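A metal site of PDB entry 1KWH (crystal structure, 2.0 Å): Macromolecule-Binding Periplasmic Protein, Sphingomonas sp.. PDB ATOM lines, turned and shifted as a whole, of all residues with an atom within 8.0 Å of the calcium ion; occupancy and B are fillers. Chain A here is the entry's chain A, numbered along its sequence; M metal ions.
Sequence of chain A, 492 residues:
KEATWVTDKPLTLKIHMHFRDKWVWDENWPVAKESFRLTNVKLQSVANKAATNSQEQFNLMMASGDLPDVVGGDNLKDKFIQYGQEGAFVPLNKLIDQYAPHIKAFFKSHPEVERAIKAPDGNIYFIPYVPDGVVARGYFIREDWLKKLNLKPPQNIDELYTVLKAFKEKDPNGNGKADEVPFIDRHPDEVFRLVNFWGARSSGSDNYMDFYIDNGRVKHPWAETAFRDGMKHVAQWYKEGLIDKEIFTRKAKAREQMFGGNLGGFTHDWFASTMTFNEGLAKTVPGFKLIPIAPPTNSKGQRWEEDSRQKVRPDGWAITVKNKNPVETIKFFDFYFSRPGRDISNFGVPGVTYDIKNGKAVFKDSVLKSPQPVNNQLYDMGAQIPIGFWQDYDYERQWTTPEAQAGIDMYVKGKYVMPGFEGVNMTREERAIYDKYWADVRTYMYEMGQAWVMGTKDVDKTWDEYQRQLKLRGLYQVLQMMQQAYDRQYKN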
ATOM      1  N   TRP A 145      32.033 -18.946 -24.293  1.00  0.00           N
ATOM      2  CA  TRP A 145      30.596 -18.732 -24.383  1.00  0.00           C
ATOM      3  C   TRP A 145      30.023 -19.718 -25.383  1.00  0.00           C
ATOM      4  O   TRP A 145      28.975 -20.306 -25.139  1.00  0.00           O
ATOM      5  CB  TRP A 145      30.288 -17.292 -24.800  1.00  0.00           C
ATOM      6  CG  TRP A 145      30.343 -16.325 -23.642  1.00  0.00           C
ATOM      7  CD1 TRP A 145      30.807 -16.590 -22.389  1.00  0.00           C
ATOM      8  CD2 TRP A 145      29.922 -14.961 -23.645  1.00  0.00           C
ATOM      9  NE1 TRP A 145      30.705 -15.464 -21.600  1.00  0.00           N
ATOM     10  CE2 TRP A 145      30.161 -14.452 -22.345  1.00  0.00           C
ATOM     11  CE3 TRP A 145      29.368 -14.108 -24.609  1.00  0.00           C
ATOM     12  CZ2 TRP A 145      29.867 -13.124 -21.990  1.00  0.00           C
ATOM     13  CZ3 TRP A 145      29.074 -12.790 -24.256  1.00  0.00           C
ATOM     14  CH2 TRP A 145      29.328 -12.311 -22.955  1.00  0.00           C
ATOM     15  N   PHE A 167      24.030 -15.302 -27.718  1.00  0.00           N
ATOM     16  CA  PHE A 167      24.833 -14.557 -26.760  1.00  0.00           C
ATOM     17  C   PHE A 167      23.976 -13.577 -25.968  1.00  0.00           C
ATOM     18  O   PHE A 167      24.167 -13.399 -24.769  1.00  0.00           O
ATOM     19  CB  PHE A 167      25.944 -13.764 -27.463  1.00  0.00           C
ATOM     20  CG  PHE A 167      27.153 -14.575 -27.822  1.00  0.00           C
ATOM     21  CD1 PHE A 167      27.170 -15.951 -27.665  1.00  0.00           C
ATOM     22  CD2 PHE A 167      28.280 -13.940 -28.358  1.00  0.00           C
ATOM     23  CE1 PHE A 167      28.294 -16.703 -28.039  1.00  0.00           C
ATOM     24  CE2 PHE A 167      29.403 -14.673 -28.729  1.00  0.00           C
ATOM     25  CZ  PHE A 167      29.410 -16.059 -28.570  1.00  0.00           C
ATOM     26  N   LYS A 168      23.038 -12.917 -26.637  1.00  0.00           N
ATOM     27  CA  LYS A 168      22.192 -11.944 -25.955  1.00  0.00           C
ATOM     28  C   LYS A 168      20.999 -12.542 -25.232  1.00  0.00           C
ATOM     29  O   LYS A 168      20.528 -11.988 -24.236  1.00  0.00           O
ATOM     30  CB  LYS A 168      21.699 -10.888 -26.942  1.00  0.00           C
ATOM     31  CG  LYS A 168      20.757  -9.884 -26.288  1.00  0.00           C
ATOM     32  CD  LYS A 168      20.658  -8.585 -27.031  1.00  0.00           C
ATOM     33  CE  LYS A 168      20.002  -7.543 -26.129  1.00  0.00           C
ATOM     34  NZ  LYS A 168      18.737  -8.080 -25.521  1.00  0.00           N
ATOM     35  N   GLU A 169      20.503 -13.670 -25.730  1.00  0.00           N
ATOM     36  CA  GLU A 169      19.327 -14.298 -25.146  1.00  0.00           C
ATOM     37  C   GLU A 169      19.560 -15.427 -24.146  1.00  0.00           C
ATOM     38  O   GLU A 169      18.815 -15.544 -23.172  1.00  0.00           O
ATOM     39  CB  GLU A 169      18.411 -14.799 -26.277  1.00  0.00           C
ATOM     40  CG  GLU A 169      17.908 -13.686 -27.197  1.00  0.00           C
ATOM     41  CD  GLU A 169      17.296 -14.212 -28.491  1.00  0.00           C
ATOM     42  OE1 GLU A 169      16.894 -13.394 -29.339  1.00  0.00           O
ATOM     43  OE2 GLU A 169      17.228 -15.449 -28.674  1.00  0.00           O
ATOM     44  N   LYS A 170      20.573 -16.262 -24.363  1.00  0.00           N
ATOM     45  CA  LYS A 170      20.821 -17.399 -23.465  1.00  0.00           C
ATOM     46  C   LYS A 170      21.805 -17.234 -22.323  1.00  0.00           C
ATOM     47  O   LYS A 170      22.482 -18.183 -21.927  1.00  0.00           O
ATOM     48  CB  LYS A 170      21.172 -18.629 -24.309  1.00  0.00           C
ATOM     49  CG  LYS A 170      20.106 -18.913 -25.353  1.00  0.00           C
ATOM     50  CD  LYS A 170      20.338 -20.214 -26.099  1.00  0.00           C
ATOM     51  CE  LYS A 170      19.184 -20.469 -27.067  1.00  0.00           C
ATOM     52  NZ  LYS A 170      19.256 -21.816 -27.698  1.00  0.00           N
ATOM     53  N   ASP A 171      21.872 -16.022 -21.783  1.00  0.00           N
ATOM     54  CA  ASP A 171      22.729 -15.692 -20.644  1.00  0.00           C
ATOM     55  C   ASP A 171      24.027 -16.493 -20.539  1.00  0.00           C
ATOM     56  O   ASP A 171      24.168 -17.336 -19.659  1.00  0.00           O
ATOM     57  CB  ASP A 171      21.928 -15.881 -19.347  1.00  0.00           C
ATOM     58  CG  ASP A 171      22.632 -15.288 -18.143  1.00  0.00           C
ATOM     59  OD1 ASP A 171      22.223 -15.611 -17.003  1.00  0.00           O
ATOM     60  OD2 ASP A 171      23.573 -14.494 -18.335  1.00  0.00           O
ATOM     61  N   PRO A 172      24.998 -16.234 -21.428  1.00  0.00           N
ATOM     62  CA  PRO A 172      26.250 -16.981 -21.352  1.00  0.00           C
ATOM     63  C   PRO A 172      27.040 -16.707 -20.065  1.00  0.00           C
ATOM     64  O   PRO A 172      27.662 -17.620 -19.517  1.00  0.00           O
ATOM     65  CB  PRO A 172      26.987 -16.557 -22.616  1.00  0.00           C
ATOM     66  CG  PRO A 172      26.502 -15.153 -22.826  1.00  0.00           C
ATOM     67  CD  PRO A 172      25.022 -15.284 -22.563  1.00  0.00           C
ATOM     68  N   ASN A 173      27.035 -15.468 -19.582  1.00  0.00           N
ATOM     69  CA  ASN A 173      27.777 -15.185 -18.353  1.00  0.00           C
ATOM     70  C   ASN A 173      26.973 -15.713 -17.152  1.00  0.00           C
ATOM     71  O   ASN A 173      27.409 -15.617 -16.013  1.00  0.00           O
ATOM     72  CB  ASN A 173      28.096 -13.689 -18.198  1.00  0.00           C
ATOM     73  CG  ASN A 173      26.881 -12.818 -17.975  1.00  0.00           C
ATOM     74  OD1 ASN A 173      25.813 -13.289 -17.564  1.00  0.00           O
ATOM     75  ND2 ASN A 173      27.038 -11.514 -18.221  1.00  0.00           N
ATOM     76  N   GLY A 174      25.804 -16.254 -17.457  1.00  0.00           N
ATOM     77  CA  GLY A 174      24.929 -16.837 -16.457  1.00  0.00           C
ATOM     78  C   GLY A 174      24.612 -16.099 -15.165  1.00  0.00           C
ATOM     79  O   GLY A 174      24.403 -16.763 -14.142  1.00  0.00           O
ATOM     80  N   ASN A 175      24.561 -14.779 -15.174  1.00  0.00           N
ATOM     81  CA  ASN A 175      24.217 -14.059 -13.951  1.00  0.00           C
ATOM     82  C   ASN A 175      22.720 -13.772 -13.922  1.00  0.00           C
ATOM     83  O   ASN A 175      22.258 -12.804 -13.329  1.00  0.00           O
ATOM     84  CB  ASN A 175      25.008 -12.736 -13.837  1.00  0.00           C
ATOM     85  CG  ASN A 175      24.683 -11.757 -14.932  1.00  0.00           C
ATOM     86  OD1 ASN A 175      23.546 -11.651 -15.380  1.00  0.00           O
ATOM     87  ND2 ASN A 175      25.687 -11.009 -15.366  1.00  0.00           N
ATOM     88  N   GLY A 176      21.965 -14.647 -14.590  1.00  0.00           N
ATOM     89  CA  GLY A 176      20.521 -14.516 -14.629  1.00  0.00           C
ATOM     90  C   GLY A 176      20.011 -13.203 -15.189  1.00  0.00           C
ATOM     91  O   GLY A 176      18.871 -12.826 -14.934  1.00  0.00           O
ATOM     92  N   LYS A 177      20.847 -12.502 -15.941  1.00  0.00           N
ATOM     93  CA  LYS A 177      20.461 -11.226 -16.525  1.00  0.00           C
ATOM     94  C   LYS A 177      20.730 -11.175 -18.025  1.00  0.00           C
ATOM     95  O   LYS A 177      21.611 -11.867 -18.525  1.00  0.00           O
ATOM     96  CB  LYS A 177      21.212 -10.075 -15.857  1.00  0.00           C
ATOM     97  CG  LYS A 177      20.939  -9.898 -14.376  1.00  0.00           C
ATOM     98  CD  LYS A 177      21.793  -8.771 -13.798  1.00  0.00           C
ATOM     99  CE  LYS A 177      21.537  -7.454 -14.531  1.00  0.00           C
ATOM    100  NZ  LYS A 177      22.348  -6.313 -13.989  1.00  0.00           N
ATOM    101  N   ALA A 178      19.970 -10.342 -18.726  1.00  0.00           N
ATOM    102  CA  ALA A 178      20.160 -10.177 -20.158  1.00  0.00           C
ATOM    103  C   ALA A 178      21.033  -8.935 -20.308  1.00  0.00           C
ATOM    104  O   ALA A 178      20.612  -7.931 -20.880  1.00  0.00           O
ATOM    105  CB  ALA A 178      18.814  -9.971 -20.852  1.00  0.00           C
ATOM    106  N   ASP A 179      22.254  -9.023 -19.777  1.00  0.00           N
ATOM    107  CA  ASP A 179      23.202  -7.917 -19.838  1.00  0.00           C
ATOM    108  C   ASP A 179      24.280  -8.092 -20.918  1.00  0.00           C
ATOM    109  O   ASP A 179      25.165  -7.250 -21.063  1.00  0.00           O
ATOM    110  CB  ASP A 179      23.891  -7.739 -18.474  1.00  0.00           C
ATOM    111  CG  ASP A 179      24.566  -9.015 -17.980  1.00  0.00           C
ATOM    112  OD1 ASP A 179      25.461  -8.922 -17.111  1.00  0.00           O
ATOM    113  OD2 ASP A 179      24.210 -10.109 -18.451  1.00  0.00           O
ATOM    114  N   GLU A 180      24.201  -9.189 -21.667  1.00  0.00           N
ATOM    115  CA  GLU A 180      25.185  -9.449 -22.713  1.00  0.00           C
ATOM    116  C   GLU A 180      25.087  -8.533 -23.922  1.00  0.00           C
ATOM    117  O   GLU A 180      23.997  -8.192 -24.393  1.00  0.00           O
ATOM    118  CB  GLU A 180      25.106 -10.911 -23.191  1.00  0.00           C
ATOM    119  CG  GLU A 180      25.635 -11.943 -22.211  1.00  0.00           C
ATOM    120  CD  GLU A 180      24.618 -12.335 -21.141  1.00  0.00           C
ATOM    121  OE1 GLU A 180      24.963 -13.171 -20.279  1.00  0.00           O
ATOM    122  OE2 GLU A 180      23.481 -11.824 -21.181  1.00  0.00           O
ATOM    123  N   VAL A 181      26.241  -8.108 -24.422  1.00  0.00           N
ATOM    124  CA  VAL A 181      26.298  -7.250 -25.595  1.00  0.00           C
ATOM    125  C   VAL A 181      27.184  -8.000 -26.587  1.00  0.00           C
ATOM    126  O   VAL A 181      28.416  -7.942 -26.499  1.00  0.00           O
ATOM    127  CB  VAL A 181      26.918  -5.885 -25.250  1.00  0.00           C
ATOM    128  CG1 VAL A 181      26.902  -4.989 -26.478  1.00  0.00           C
ATOM    129  CG2 VAL A 181      26.138  -5.239 -24.119  1.00  0.00           C
ATOM    130  N   ASN A 262      32.848  -8.916 -18.661  1.00  0.00           N
ATOM    131  CA  ASN A 262      32.273 -10.163 -19.158  1.00  0.00           C
ATOM    132  C   ASN A 262      30.893  -9.953 -19.787  1.00  0.00           C
ATOM    133  O   ASN A 262      29.964 -10.739 -19.585  1.00  0.00           O
ATOM    134  CB  ASN A 262      32.212 -11.182 -18.003  1.00  0.00           C
ATOM    135  CG  ASN A 262      31.701 -12.531 -18.433  1.00  0.00           C
ATOM    136  OD1 ASN A 262      32.109 -13.073 -19.460  1.00  0.00           O
ATOM    137  ND2 ASN A 262      30.796 -13.102 -17.644  1.00  0.00           N
ATOM    138  N   LEU A 263      30.769  -8.882 -20.576  1.00  0.00           N
ATOM    139  CA  LEU A 263      29.530  -8.517 -21.261  1.00  0.00           C
ATOM    140  C   LEU A 263      29.562  -8.819 -22.765  1.00  0.00           C
ATOM    141  O   LEU A 263      28.588  -9.323 -23.326  1.00  0.00           O
ATOM    142  CB  LEU A 263      29.251  -7.019 -21.070  1.00  0.00           C
ATOM    143  CG  LEU A 263      28.798  -6.469 -19.718  1.00  0.00           C
ATOM    144  CD1 LEU A 263      29.752  -6.900 -18.627  1.00  0.00           C
ATOM    145  CD2 LEU A 263      28.748  -4.961 -19.787  1.00  0.00           C
HETATM  146 CA    CA M   1      23.741 -12.317 -18.248  1.00  0.00          CA
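The side-chain carboxylate (OD2) of Asp 171 is bound to the calcium ion. The calcium ion is bound by the backbone carbonyl oxygen (O) of Lys 177, at 2.2 Å. The side-chain carboxylate (OD2) of Asp 179 is bound to the calcium ion, at 2.3 Å. The calcium ion is bound by OD1 of Asn 173, 2.4 Å away. The calcium ion is bound by the side-chain carboxylate (OE1) of Glu 180, 2.5 Å away. Slightly farther from the calcium ion lies the side-chain amide oxygen (OD1) of Asn 175 (3.0 Å). Slightly farther from the calcium ion lies OE2 of Glu 180 (3.0 Å).
The nearest printed residue that does not touch the calcium ion is Ala 178 (4.3 Å).
The side-chain carboxylate (OD1) of Asp 171 is in hydrogen-bond range of the backbone NH (N) of Asn 175, at 3.1 Å. OD2 of Asp 171 lies close to N of Gly 174. OD1 of Asp 171 lies within hydrogen-bond range of N of Gly 176, at 2.6 Å. The side-chain amide oxygen of Asn 175 lies close to the backbone NH of Lys 177, 2.9 Å away. The side-chain amide nitrogen of Asn 175 sits at hydrogen-bond distance from the side-chain carboxylate of Asp 179, at 2.7 Å. The side-chain amide nitrogen (ND2) of Asn 173 sits close to the side-chain amide nitrogen (ND2) of Asn 175, 3.2 Å away. O of Asn 262 is in hydrogen-bond range of ND2 of Asn 173 (3.3 Å).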
